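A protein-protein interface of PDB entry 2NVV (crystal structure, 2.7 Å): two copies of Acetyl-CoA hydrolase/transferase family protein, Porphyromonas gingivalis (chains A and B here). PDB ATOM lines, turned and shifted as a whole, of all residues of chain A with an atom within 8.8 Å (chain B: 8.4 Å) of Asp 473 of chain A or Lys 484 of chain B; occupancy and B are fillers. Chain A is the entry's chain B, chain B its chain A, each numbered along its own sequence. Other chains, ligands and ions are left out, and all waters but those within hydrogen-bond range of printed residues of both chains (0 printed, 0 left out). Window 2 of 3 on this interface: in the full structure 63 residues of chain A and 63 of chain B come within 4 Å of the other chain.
The backbone carbonyl oxygen of Leu 472 of chain B sits close to the side-chain amide oxygen of Gln 480 of chain A, 3.4 Å away. The side-chain amide oxygen of Gln 480 of chain A lies close to the side-chain carboxylate of Asp 473 of chain B (2.8 Å). OE1 of Gln 480 of chain B lies close to O of Leu 472 of chain A (3.4 Å). The side-chain carboxylate (OD1) of Asp 473 of chain A sits close to the side-chain amide oxygen (OE1) of Gln 480 of chain B (2.9 Å). The side-chain amino group of Lys 484 of chain B lies within salt-bridge range of the side-chain carboxylate of Asp 473 of chain A, at 3.9 Å.
The backbone carbonyl oxygen of Gln 480 of chain B sits close to the side-chain amino group of Lys 484 of chain B, at 3.1 Å. The side-chain amide oxygen (OD1) of Asn 471 of chain A sits close to the backbone NH (N) of Asp 473 of chain A (3.0 Å).
Met 408 of chain A touches Phe 476 of chain B (SD to CZ, 3.7 Å). CD1 of Phe 476 of chain B touches CG of Leu 472 of chain A, at 3.7 Å. CD2 of Leu 472 of chain A touches CB of His 479 of chain B, 3.6 Å away. Cys 475 of chain A touches Phe 476 of chain B. Phe 476 of chain A touches Leu 472 of chain B (CD1 to CG, 3.7 Å). Phe 476 of chain B touches Phe 476 of chain A.
Of chain B, only Gln 480 (2.9 Å) and Lys 484 (3.9 Å) come within 4 Å of Asp 473 of chain A. Lys 484 of chain B touches just one residue of chain A: Asp 473 (3.9 Å). No residue of chain A comes within 4 Å of Ala 483 of chain B. No residue of chain A comes within 4 Å of Ser 485 of chain B. Printed residues of chain B within 4 Å of Met 408 of chain A: Phe 476 (3.7 Å). Of the printed residues of chain B, Gln 480 of chain A touches Leu 472 (3.4 Å) and Asp 473 (2.8 Å). The nearest residue of chain B that does not touch Asp 473 of chain A is Phe 476 of chain B (5.9 Å). The nearest residue of chain A that does not touch Lys 484 of chain B is Leu 472 of chain A (7.3 Å).
Of the 19 printed residues of chain B, 6 touch a printed residue of chain A. Printed residues of chain B that touch a printed residue of chain A: Leu 472, Asp 473, Phe 476, His 479, Gln 480 and Lys 484. Hydrophobic or aromatic side chains of chain B that line the printed part of chain A: Leu 472, Phe 476 and His 479. Of the 17 printed residues of chain A, 6 touch a printed residue of chain B. Hydrophobic or aromatic side chains of chain A within 4 Å of the printed part of chain B: Met 408, Leu 472 and Phe 476. Among the printed residues, 11 pairs touch across the chains. Among the printed residues, Asp or Glu carboxylates within 4 Å of a Lys or Arg side-chain nitrogen of the other chain: Asp 473 of chain A with Lys 484 of chain B (3.9 Å).
Leu 472 of chain A touches Phe 476 of chain B, and with the chains exchanged Phe 476 of chain A touches Leu 472 of chain B. Leu 472 of chain A touches Gln 480 of chain B, and with the chains exchanged Gln 480 of chain A touches Leu 472 of chain B. Asp 473 of chain A touches Gln 480 of chain B, and with the chains exchanged Gln 480 of chain A touches Asp 473 of chain B. Phe 476 of chain A touches its own counterpart, Phe 476 of chain B. Positions printed for both chains: 472, 473, 474, 476, 477, 480 and 496. Of the 11 pairs that touch across the chains among the printed residues, 7 have their exchanged pair printed and touching as well.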
ATOM      1  N   MET A 408      14.902 -31.479 -36.439  1.00  0.00           N
ATOM      2  CA  MET A 408      14.112 -30.812 -37.473  1.00  0.00           C
ATOM      3  C   MET A 408      15.009 -29.776 -38.149  1.00  0.00           C
ATOM      4  O   MET A 408      15.757 -29.067 -37.466  1.00  0.00           O
ATOM      5  CB  MET A 408      12.902 -30.106 -36.861  1.00  0.00           C
ATOM      6  CG  MET A 408      11.942 -29.558 -37.907  1.00  0.00           C
ATOM      7  SD  MET A 408      10.599 -28.290 -37.224  1.00  0.00           S
ATOM      8  CE  MET A 408       9.231 -29.571 -36.697  1.00  0.00           C
ATOM      9  N   TYR A 459      15.525 -38.628 -28.770  1.00  0.00           N
ATOM     10  CA  TYR A 459      14.536 -37.680 -29.253  1.00  0.00           C
ATOM     11  C   TYR A 459      13.264 -38.400 -29.687  1.00  0.00           C
ATOM     12  O   TYR A 459      12.158 -37.862 -29.566  1.00  0.00           O
ATOM     13  CB  TYR A 459      15.087 -36.894 -30.442  1.00  0.00           C
ATOM     14  CG  TYR A 459      14.120 -35.850 -30.951  1.00  0.00           C
ATOM     15  CD1 TYR A 459      13.884 -34.668 -30.234  1.00  0.00           C
ATOM     16  CD2 TYR A 459      13.409 -36.051 -32.136  1.00  0.00           C
ATOM     17  CE1 TYR A 459      12.964 -33.722 -30.695  1.00  0.00           C
ATOM     18  CE2 TYR A 459      12.482 -35.108 -32.599  1.00  0.00           C
ATOM     19  CZ  TYR A 459      12.272 -33.952 -31.875  1.00  0.00           C
ATOM     20  OH  TYR A 459      11.378 -33.016 -32.332  1.00  0.00           O
ATOM     21  N   LEU A 462      10.527 -39.250 -26.623  1.00  0.00           N
ATOM     22  CA  LEU A 462      10.122 -38.179 -25.715  1.00  0.00           C
ATOM     23  C   LEU A 462       8.616 -38.131 -25.447  1.00  0.00           C
ATOM     24  O   LEU A 462       8.096 -37.137 -24.936  1.00  0.00           O
ATOM     25  CB  LEU A 462      10.608 -36.821 -26.237  1.00  0.00           C
ATOM     26  CG  LEU A 462      12.132 -36.676 -26.287  1.00  0.00           C
ATOM     27  CD1 LEU A 462      12.516 -35.243 -26.670  1.00  0.00           C
ATOM     28  CD2 LEU A 462      12.725 -37.055 -24.921  1.00  0.00           C
ATOM     29  N   VAL A 464       6.075 -38.116 -27.659  1.00  0.00           N
ATOM     30  CA  VAL A 464       5.224 -37.516 -28.688  1.00  0.00           C
ATOM     31  C   VAL A 464       4.383 -38.551 -29.437  1.00  0.00           C
ATOM     32  O   VAL A 464       4.885 -39.585 -29.871  1.00  0.00           O
ATOM     33  CB  VAL A 464       6.050 -36.710 -29.713  1.00  0.00           C
ATOM     34  CG1 VAL A 464       5.133 -36.148 -30.795  1.00  0.00           C
ATOM     35  CG2 VAL A 464       6.771 -35.570 -29.014  1.00  0.00           C
ATOM     36  N   GLN A 470       7.669 -35.277 -33.841  1.00  0.00           N
ATOM     37  CA  GLN A 470       8.365 -34.003 -33.647  1.00  0.00           C
ATOM     38  C   GLN A 470       7.904 -33.380 -32.340  1.00  0.00           C
ATOM     39  O   GLN A 470       6.703 -33.298 -32.071  1.00  0.00           O
ATOM     40  CB  GLN A 470       8.095 -33.040 -34.815  1.00  0.00           C
ATOM     41  CG  GLN A 470       8.905 -33.348 -36.069  1.00  0.00           C
ATOM     42  CD  GLN A 470      10.382 -32.972 -35.935  1.00  0.00           C
ATOM     43  OE1 GLN A 470      10.937 -32.950 -34.839  1.00  0.00           O
ATOM     44  NE2 GLN A 470      11.021 -32.686 -37.059  1.00  0.00           N
ATOM     45  N   ASN A 471       8.860 -32.963 -31.516  1.00  0.00           N
ATOM     46  CA  ASN A 471       8.529 -32.335 -30.245  1.00  0.00           C
ATOM     47  C   ASN A 471       8.712 -30.821 -30.363  1.00  0.00           C
ATOM     48  O   ASN A 471       9.814 -30.299 -30.190  1.00  0.00           O
ATOM     49  CB  ASN A 471       9.419 -32.880 -29.138  1.00  0.00           C
ATOM     50  CG  ASN A 471       8.927 -32.487 -27.770  1.00  0.00           C
ATOM     51  OD1 ASN A 471       8.646 -31.319 -27.520  1.00  0.00           O
ATOM     52  ND2 ASN A 471       8.812 -33.462 -26.871  1.00  0.00           N
ATOM     53  N   LEU A 472       7.619 -30.125 -30.657  1.00  0.00           N
ATOM     54  CA  LEU A 472       7.641 -28.683 -30.834  1.00  0.00           C
ATOM     55  C   LEU A 472       8.270 -27.880 -29.700  1.00  0.00           C
ATOM     56  O   LEU A 472       8.593 -26.706 -29.882  1.00  0.00           O
ATOM     57  CB  LEU A 472       6.218 -28.180 -31.126  1.00  0.00           C
ATOM     58  CG  LEU A 472       5.880 -27.997 -32.620  1.00  0.00           C
ATOM     59  CD1 LEU A 472       6.318 -29.211 -33.434  1.00  0.00           C
ATOM     60  CD2 LEU A 472       4.383 -27.741 -32.772  1.00  0.00           C
ATOM     61  N   ASP A 473       8.449 -28.505 -28.539  1.00  0.00           N
ATOM     62  CA  ASP A 473       9.068 -27.829 -27.398  1.00  0.00           C
ATOM     63  C   ASP A 473      10.590 -27.793 -27.484  1.00  0.00           C
ATOM     64  O   ASP A 473      11.222 -26.904 -26.905  1.00  0.00           O
ATOM     65  CB  ASP A 473       8.693 -28.506 -26.070  1.00  0.00           C
ATOM     66  CG  ASP A 473       7.285 -28.184 -25.618  1.00  0.00           C
ATOM     67  OD1 ASP A 473       6.740 -27.135 -26.024  1.00  0.00           O
ATOM     68  OD2 ASP A 473       6.720 -28.970 -24.837  1.00  0.00           O
ATOM     69  N   CYS A 474      11.167 -28.747 -28.213  1.00  0.00           N
ATOM     70  CA  CYS A 474      12.625 -28.853 -28.324  1.00  0.00           C
ATOM     71  C   CYS A 474      13.200 -29.355 -29.651  1.00  0.00           C
ATOM     72  O   CYS A 474      14.369 -29.753 -29.701  1.00  0.00           O
ATOM     73  CB  CYS A 474      13.141 -29.761 -27.205  1.00  0.00           C
ATOM     74  SG  CYS A 474      12.314 -31.381 -27.188  1.00  0.00           S
ATOM     75  N   CYS A 475      12.411 -29.343 -30.720  1.00  0.00           N
ATOM     76  CA  CYS A 475      12.909 -29.810 -32.015  1.00  0.00           C
ATOM     77  C   CYS A 475      14.114 -29.002 -32.518  1.00  0.00           C
ATOM     78  O   CYS A 475      14.871 -29.470 -33.368  1.00  0.00           O
ATOM     79  CB  CYS A 475      11.782 -29.792 -33.061  1.00  0.00           C
ATOM     80  SG  CYS A 475      10.911 -28.211 -33.263  1.00  0.00           S
ATOM     81  N   PHE A 476      14.293 -27.792 -31.994  1.00  0.00           N
ATOM     82  CA  PHE A 476      15.419 -26.942 -32.399  1.00  0.00           C
ATOM     83  C   PHE A 476      16.508 -26.807 -31.331  1.00  0.00           C
ATOM     84  O   PHE A 476      17.350 -25.910 -31.396  1.00  0.00           O
ATOM     85  CB  PHE A 476      14.917 -25.551 -32.798  1.00  0.00           C
ATOM     86  CG  PHE A 476      14.145 -25.535 -34.092  1.00  0.00           C
ATOM     87  CD1 PHE A 476      12.966 -24.803 -34.204  1.00  0.00           C
ATOM     88  CD2 PHE A 476      14.593 -26.249 -35.196  1.00  0.00           C
ATOM     89  CE1 PHE A 476      12.248 -24.783 -35.394  1.00  0.00           C
ATOM     90  CE2 PHE A 476      13.883 -26.236 -36.389  1.00  0.00           C
ATOM     91  CZ  PHE A 476      12.712 -25.505 -36.491  1.00  0.00           C
ATOM     92  N   ALA A 477      16.498 -27.706 -30.355  1.00  0.00           N
ATOM     93  CA  ALA A 477      17.488 -27.695 -29.287  1.00  0.00           C
ATOM     94  C   ALA A 477      18.931 -27.768 -29.824  1.00  0.00           C
ATOM     95  O   ALA A 477      19.839 -27.135 -29.282  1.00  0.00           O
ATOM     96  CB  ALA A 477      17.227 -28.846 -28.341  1.00  0.00           C
ATOM     97  N   GLN A 480      19.723 -24.400 -31.069  1.00  0.00           N
ATOM     98  CA  GLN A 480      19.739 -23.528 -29.908  1.00  0.00           C
ATOM     99  C   GLN A 480      21.008 -23.742 -29.098  1.00  0.00           C
ATOM    100  O   GLN A 480      21.637 -22.781 -28.669  1.00  0.00           O
ATOM    101  CB  GLN A 480      18.515 -23.794 -29.033  1.00  0.00           C
ATOM    102  CG  GLN A 480      17.234 -23.184 -29.577  1.00  0.00           C
ATOM    103  CD  GLN A 480      16.031 -23.519 -28.728  1.00  0.00           C
ATOM    104  OE1 GLN A 480      15.078 -22.745 -28.649  1.00  0.00           O
ATOM    105  NE2 GLN A 480      16.060 -24.686 -28.090  1.00  0.00           N
ATOM    106  N   TRP A 493      17.991 -33.482 -23.416  1.00  0.00           N
ATOM    107  CA  TRP A 493      16.572 -33.218 -23.564  1.00  0.00           C
ATOM    108  C   TRP A 493      15.879 -32.765 -22.295  1.00  0.00           C
ATOM    109  O   TRP A 493      14.913 -32.004 -22.357  1.00  0.00           O
ATOM    110  CB  TRP A 493      15.887 -34.450 -24.149  1.00  0.00           C
ATOM    111  CG  TRP A 493      16.487 -34.823 -25.471  1.00  0.00           C
ATOM    112  CD1 TRP A 493      17.177 -35.962 -25.769  1.00  0.00           C
ATOM    113  CD2 TRP A 493      16.519 -34.016 -26.658  1.00  0.00           C
ATOM    114  NE1 TRP A 493      17.643 -35.918 -27.061  1.00  0.00           N
ATOM    115  CE2 TRP A 493      17.257 -34.735 -27.633  1.00  0.00           C
ATOM    116  CE3 TRP A 493      15.998 -32.754 -26.993  1.00  0.00           C
ATOM    117  CZ2 TRP A 493      17.490 -34.237 -28.920  1.00  0.00           C
ATOM    118  CZ3 TRP A 493      16.228 -32.256 -28.280  1.00  0.00           C
ATOM    119  CH2 TRP A 493      16.969 -33.000 -29.227  1.00  0.00           C
ATOM    120  N   ASP A 495      16.986 -30.788 -20.309  1.00  0.00           N
ATOM    121  CA  ASP A 495      17.337 -29.379 -20.168  1.00  0.00           C
ATOM    122  C   ASP A 495      16.472 -28.524 -21.066  1.00  0.00           C
ATOM    123  O   ASP A 495      16.196 -27.368 -20.752  1.00  0.00           O
ATOM    124  CB  ASP A 495      18.805 -29.141 -20.530  1.00  0.00           C
ATOM    125  CG  ASP A 495      19.766 -29.680 -19.486  1.00  0.00           C
ATOM    126  OD1 ASP A 495      20.979 -29.740 -19.777  1.00  0.00           O
ATOM    127  OD2 ASP A 495      19.321 -30.033 -18.376  1.00  0.00           O
ATOM    128  N   TYR A 496      16.052 -29.088 -22.195  1.00  0.00           N
ATOM    129  CA  TYR A 496      15.214 -28.352 -23.131  1.00  0.00           C
ATOM    130  C   TYR A 496      13.733 -28.591 -22.934  1.00  0.00           C
ATOM    131  O   TYR A 496      12.924 -28.311 -23.813  1.00  0.00           O
ATOM    132  CB  TYR A 496      15.627 -28.649 -24.571  1.00  0.00           C
ATOM    133  CG  TYR A 496      16.892 -27.909 -24.951  1.00  0.00           C
ATOM    134  CD1 TYR A 496      18.153 -28.390 -24.580  1.00  0.00           C
ATOM    135  CD2 TYR A 496      16.825 -26.682 -25.622  1.00  0.00           C
ATOM    136  CE1 TYR A 496      19.313 -27.671 -24.863  1.00  0.00           C
ATOM    137  CE2 TYR A 496      17.979 -25.953 -25.908  1.00  0.00           C
ATOM    138  CZ  TYR A 496      19.218 -26.450 -25.525  1.00  0.00           C
ATOM    139  OH  TYR A 496      20.347 -25.706 -25.788  1.00  0.00           O
ATOM    140  N   MET A 497      13.393 -29.098 -21.755  1.00  0.00           N
ATOM    141  CA  MET A 497      12.011 -29.359 -21.376  1.00  0.00           C
ATOM    142  C   MET A 497      11.983 -29.694 -19.886  1.00  0.00           C
ATOM    143  O   MET A 497      11.394 -28.895 -19.121  1.00  0.00           O
ATOM    144  CB  MET A 497      11.417 -30.512 -22.197  1.00  0.00           C
ATOM    145  CG  MET A 497      12.154 -31.839 -22.079  1.00  0.00           C
ATOM    146  SD  MET A 497      11.313 -33.281 -23.107  1.00  0.00           S
ATOM    147  CE  MET A 497      10.751 -34.410 -21.603  1.00  0.00           C
ATOM    148  N   LEU B 472      14.009 -19.326 -33.761  1.00  0.00           N
ATOM    149  CA  LEU B 472      14.003 -20.700 -33.283  1.00  0.00           C
ATOM    150  C   LEU B 472      13.628 -20.880 -31.818  1.00  0.00           C
ATOM    151  O   LEU B 472      13.313 -21.990 -31.396  1.00  0.00           O
ATOM    152  CB  LEU B 472      15.356 -21.356 -33.574  1.00  0.00           C
ATOM    153  CG  LEU B 472      15.429 -22.154 -34.887  1.00  0.00           C
ATOM    154  CD1 LEU B 472      14.805 -21.371 -36.054  1.00  0.00           C
ATOM    155  CD2 LEU B 472      16.886 -22.504 -35.171  1.00  0.00           C
ATOM    156  N   ASP B 473      13.644 -19.801 -31.043  1.00  0.00           N
ATOM    157  CA  ASP B 473      13.281 -19.896 -29.629  1.00  0.00           C
ATOM    158  C   ASP B 473      11.779 -19.894 -29.398  1.00  0.00           C
ATOM    159  O   ASP B 473      11.319 -20.406 -28.373  1.00  0.00           O
ATOM    160  CB  ASP B 473      13.869 -18.746 -28.819  1.00  0.00           C
ATOM    161  CG  ASP B 473      15.352 -18.892 -28.581  1.00  0.00           C
ATOM    162  OD1 ASP B 473      15.844 -20.042 -28.539  1.00  0.00           O
ATOM    163  OD2 ASP B 473      16.023 -17.851 -28.411  1.00  0.00           O
ATOM    164  N   CYS B 474      11.022 -19.335 -30.346  1.00  0.00           N
ATOM    165  CA  CYS B 474       9.568 -19.234 -30.208  1.00  0.00           C
ATOM    166  C   CYS B 474       8.727 -19.353 -31.485  1.00  0.00           C
ATOM    167  O   CYS B 474       7.540 -19.019 -31.470  1.00  0.00           O
ATOM    168  CB  CYS B 474       9.226 -17.912 -29.509  1.00  0.00           C
ATOM    169  SG  CYS B 474       9.952 -16.424 -30.272  1.00  0.00           S
ATOM    170  N   PHE B 476       7.278 -21.696 -32.692  1.00  0.00           N
ATOM    171  CA  PHE B 476       6.141 -22.588 -32.474  1.00  0.00           C
ATOM    172  C   PHE B 476       5.287 -22.203 -31.279  1.00  0.00           C
ATOM    173  O   PHE B 476       4.495 -23.008 -30.787  1.00  0.00           O
ATOM    174  CB  PHE B 476       6.622 -24.029 -32.304  1.00  0.00           C
ATOM    175  CG  PHE B 476       7.150 -24.647 -33.574  1.00  0.00           C
ATOM    176  CD1 PHE B 476       8.318 -25.408 -33.564  1.00  0.00           C
ATOM    177  CD2 PHE B 476       6.474 -24.474 -34.774  1.00  0.00           C
ATOM    178  CE1 PHE B 476       8.798 -25.985 -34.733  1.00  0.00           C
ATOM    179  CE2 PHE B 476       6.950 -25.052 -35.945  1.00  0.00           C
ATOM    180  CZ  PHE B 476       8.112 -25.808 -35.925  1.00  0.00           C
ATOM    181  N   ALA B 477       5.435 -20.966 -30.820  1.00  0.00           N
ATOM    182  CA  ALA B 477       4.667 -20.470 -29.686  1.00  0.00           C
ATOM    183  C   ALA B 477       3.158 -20.568 -29.913  1.00  0.00           C
ATOM    184  O   ALA B 477       2.406 -20.857 -28.987  1.00  0.00           O
ATOM    185  CB  ALA B 477       5.054 -19.034 -29.408  1.00  0.00           C
ATOM    186  N   PHE B 478       2.710 -20.309 -31.135  1.00  0.00           N
ATOM    187  CA  PHE B 478       1.290 -20.388 -31.460  1.00  0.00           C
ATOM    188  C   PHE B 478       0.740 -21.788 -31.164  1.00  0.00           C
ATOM    189  O   PHE B 478      -0.286 -21.939 -30.504  1.00  0.00           O
ATOM    190  CB  PHE B 478       1.074 -20.044 -32.938  1.00  0.00           C
ATOM    191  CG  PHE B 478       0.859 -18.579 -33.196  1.00  0.00           C
ATOM    192  CD1 PHE B 478       1.617 -17.621 -32.531  1.00  0.00           C
ATOM    193  CD2 PHE B 478      -0.102 -18.155 -34.104  1.00  0.00           C
ATOM    194  CE1 PHE B 478       1.420 -16.257 -32.767  1.00  0.00           C
ATOM    195  CE2 PHE B 478      -0.305 -16.793 -34.345  1.00  0.00           C
ATOM    196  CZ  PHE B 478       0.461 -15.844 -33.671  1.00  0.00           C
ATOM    197  N   HIS B 479       1.444 -22.802 -31.663  1.00  0.00           N
ATOM    198  CA  HIS B 479       1.077 -24.200 -31.481  1.00  0.00           C
ATOM    199  C   HIS B 479       1.198 -24.588 -30.017  1.00  0.00           C
ATOM    200  O   HIS B 479       0.354 -25.319 -29.478  1.00  0.00           O
ATOM    201  CB  HIS B 479       2.008 -25.085 -32.301  1.00  0.00           C
ATOM    202  CG  HIS B 479       2.023 -24.757 -33.758  1.00  0.00           C
ATOM    203  ND1 HIS B 479       1.071 -25.230 -34.635  1.00  0.00           N
ATOM    204  CD2 HIS B 479       2.886 -24.021 -34.499  1.00  0.00           C
ATOM    205  CE1 HIS B 479       1.350 -24.808 -35.856  1.00  0.00           C
ATOM    206  NE2 HIS B 479       2.447 -24.073 -35.800  1.00  0.00           N
ATOM    207  N   GLN B 480       2.271 -24.115 -29.387  1.00  0.00           N
ATOM    208  CA  GLN B 480       2.510 -24.396 -27.987  1.00  0.00           C
ATOM    209  C   GLN B 480       1.413 -23.791 -27.137  1.00  0.00           C
ATOM    210  O   GLN B 480       0.929 -24.431 -26.211  1.00  0.00           O
ATOM    211  CB  GLN B 480       3.867 -23.838 -27.554  1.00  0.00           C
ATOM    212  CG  GLN B 480       5.061 -24.674 -27.988  1.00  0.00           C
ATOM    213  CD  GLN B 480       6.387 -24.031 -27.623  1.00  0.00           C
ATOM    214  OE1 GLN B 480       7.383 -24.716 -27.400  1.00  0.00           O
ATOM    215  NE2 GLN B 480       6.410 -22.708 -27.574  1.00  0.00           N
ATOM    216  N   GLU B 481       1.013 -22.560 -27.453  1.00  0.00           N
ATOM    217  CA  GLU B 481      -0.039 -21.883 -26.687  1.00  0.00           C
ATOM    218  C   GLU B 481      -1.387 -22.555 -26.851  1.00  0.00           C
ATOM    219  O   GLU B 481      -2.193 -22.555 -25.929  1.00  0.00           O
ATOM    220  CB  GLU B 481      -0.159 -20.409 -27.094  1.00  0.00           C
ATOM    221  CG  GLU B 481      -1.172 -19.633 -26.254  1.00  0.00           C
ATOM    222  CD  GLU B 481      -0.782 -19.548 -24.774  1.00  0.00           C
ATOM    223  OE1 GLU B 481      -1.685 -19.441 -23.923  1.00  0.00           O
ATOM    224  OE2 GLU B 481       0.428 -19.575 -24.461  1.00  0.00           O
ATOM    225  N   LEU B 482      -1.643 -23.126 -28.022  1.00  0.00           N
ATOM    226  CA  LEU B 482      -2.913 -23.805 -28.244  1.00  0.00           C
ATOM    227  C   LEU B 482      -3.019 -24.963 -27.272  1.00  0.00           C
ATOM    228  O   LEU B 482      -4.082 -25.233 -26.723  1.00  0.00           O
ATOM    229  CB  LEU B 482      -2.997 -24.348 -29.667  1.00  0.00           C
ATOM    230  CG  LEU B 482      -4.187 -25.271 -29.956  1.00  0.00           C
ATOM    231  CD1 LEU B 482      -5.510 -24.513 -29.752  1.00  0.00           C
ATOM    232  CD2 LEU B 482      -4.088 -25.785 -31.380  1.00  0.00           C
ATOM    233  N   ALA B 483      -1.893 -25.641 -27.068  1.00  0.00           N
ATOM    234  CA  ALA B 483      -1.808 -26.800 -26.188  1.00  0.00           C
ATOM    235  C   ALA B 483      -1.892 -26.400 -24.728  1.00  0.00           C
ATOM    236  O   ALA B 483      -2.395 -27.153 -23.893  1.00  0.00           O
ATOM    237  CB  ALA B 483      -0.510 -27.551 -26.449  1.00  0.00           C
ATOM    238  N   LYS B 484      -1.407 -25.203 -24.417  1.00  0.00           N
ATOM    239  CA  LYS B 484      -1.429 -24.719 -23.044  1.00  0.00           C
ATOM    240  C   LYS B 484      -2.760 -24.068 -22.649  1.00  0.00           C
ATOM    241  O   LYS B 484      -3.379 -24.473 -21.669  1.00  0.00           O
ATOM    242  CB  LYS B 484      -0.279 -23.734 -22.830  1.00  0.00           C
ATOM    243  CG  LYS B 484       1.034 -24.195 -23.469  1.00  0.00           C
ATOM    244  CD  LYS B 484       1.427 -25.617 -23.015  1.00  0.00           C
ATOM    245  CE  LYS B 484       1.945 -26.490 -24.171  1.00  0.00           C
ATOM    246  NZ  LYS B 484       3.217 -26.005 -24.761  1.00  0.00           N
ATOM    247  N   SER B 485      -3.203 -23.078 -23.424  1.00  0.00           N
ATOM    248  CA  SER B 485      -4.443 -22.338 -23.145  1.00  0.00           C
ATOM    249  C   SER B 485      -5.647 -22.722 -23.975  1.00  0.00           C
ATOM    250  O   SER B 485      -6.778 -22.558 -23.529  1.00  0.00           O
ATOM    251  CB  SER B 485      -4.226 -20.836 -23.344  1.00  0.00           C
ATOM    252  OG  SER B 485      -3.258 -20.332 -22.447  1.00  0.00           O
ATOM    253  N   GLY B 486      -5.409 -23.198 -25.190  1.00  0.00           N
ATOM    254  CA  GLY B 486      -6.509 -23.562 -26.063  1.00  0.00           C
ATOM    255  C   GLY B 486      -6.881 -22.378 -26.939  1.00  0.00           C
ATOM    256  O   GLY B 486      -7.804 -22.455 -27.754  1.00  0.00           O
ATOM    257  N   ASP B 487      -6.156 -21.276 -26.761  1.00  0.00           N
ATOM    258  CA  ASP B 487      -6.395 -20.059 -27.527  1.00  0.00           C
ATOM    259  C   ASP B 487      -5.060 -19.408 -27.894  1.00  0.00           C
ATOM    260  O   ASP B 487      -4.350 -18.902 -27.027  1.00  0.00           O
ATOM    261  CB  ASP B 487      -7.233 -19.074 -26.713  1.00  0.00           C
ATOM    262  CG  ASP B 487      -7.746 -17.912 -27.551  1.00  0.00           C
ATOM    263  OD1 ASP B 487      -7.003 -17.435 -28.431  1.00  0.00           O
ATOM    264  OD2 ASP B 487      -8.888 -17.470 -27.325  1.00  0.00           O
ATOM    265  N   MET B 488      -4.728 -19.407 -29.181  1.00  0.00           N
ATOM    266  CA  MET B 488      -3.468 -18.839 -29.629  1.00  0.00           C
ATOM    267  C   MET B 488      -3.338 -17.339 -29.400  1.00  0.00           C
ATOM    268  O   MET B 488      -2.234 -16.804 -29.406  1.00  0.00           O
ATOM    269  CB  MET B 488      -3.256 -19.147 -31.116  1.00  0.00           C
ATOM    270  CG  MET B 488      -3.271 -20.629 -31.465  1.00  0.00           C
ATOM    271  SD  MET B 488      -2.768 -20.939 -33.305  1.00  0.00           S
ATOM    272  CE  MET B 488      -2.260 -22.819 -33.185  1.00  0.00           C
ATOM    273  N   ASN B 490      -3.602 -15.838 -26.799  1.00  0.00           N
ATOM    274  CA  ASN B 490      -2.973 -15.635 -25.496  1.00  0.00           C
ATOM    275  C   ASN B 490      -1.455 -15.535 -25.567  1.00  0.00           C
ATOM    276  O   ASN B 490      -0.784 -15.410 -24.535  1.00  0.00           O
ATOM    277  CB  ASN B 490      -3.347 -16.766 -24.548  1.00  0.00           C
ATOM    278  CG  ASN B 490      -4.780 -16.714 -24.151  1.00  0.00           C
ATOM    279  OD1 ASN B 490      -5.306 -15.636 -23.858  1.00  0.00           O
ATOM    280  ND2 ASN B 490      -5.437 -17.868 -24.127  1.00  0.00           N
ATOM    281  N   VAL B 491      -0.914 -15.586 -26.777  1.00  0.00           N
ATOM    282  CA  VAL B 491       0.519 -15.520 -26.935  1.00  0.00           C
ATOM    283  C   VAL B 491       1.030 -14.110 -26.703  1.00  0.00           C
ATOM    284  O   VAL B 491       0.386 -13.127 -27.068  1.00  0.00           O
ATOM    285  CB  VAL B 491       0.952 -15.995 -28.351  1.00  0.00           C
ATOM    286  CG1 VAL B 491       2.412 -15.653 -28.600  1.00  0.00           C
ATOM    287  CG2 VAL B 491       0.744 -17.494 -28.490  1.00  0.00           C
ATOM    288  N   TYR B 496       7.344 -16.176 -24.318  1.00  0.00           N
ATOM    289  CA  TYR B 496       8.019 -17.289 -24.969  1.00  0.00           C
ATOM    290  C   TYR B 496       9.504 -17.049 -25.174  1.00  0.00           C
ATOM    291  O   TYR B 496      10.157 -17.712 -25.979  1.00  0.00           O
ATOM    292  CB  TYR B 496       7.328 -17.633 -26.291  1.00  0.00           C
ATOM    293  CG  TYR B 496       6.045 -18.402 -26.072  1.00  0.00           C
ATOM    294  CD1 TYR B 496       4.866 -17.750 -25.701  1.00  0.00           C
ATOM    295  CD2 TYR B 496       6.030 -19.793 -26.150  1.00  0.00           C
ATOM    296  CE1 TYR B 496       3.709 -18.470 -25.407  1.00  0.00           C
ATOM    297  CE2 TYR B 496       4.880 -20.522 -25.858  1.00  0.00           C
ATOM    298  CZ  TYR B 496       3.724 -19.858 -25.485  1.00  0.00           C
ATOM    299  OH  TYR B 496       2.596 -20.589 -25.184  1.00  0.00           O
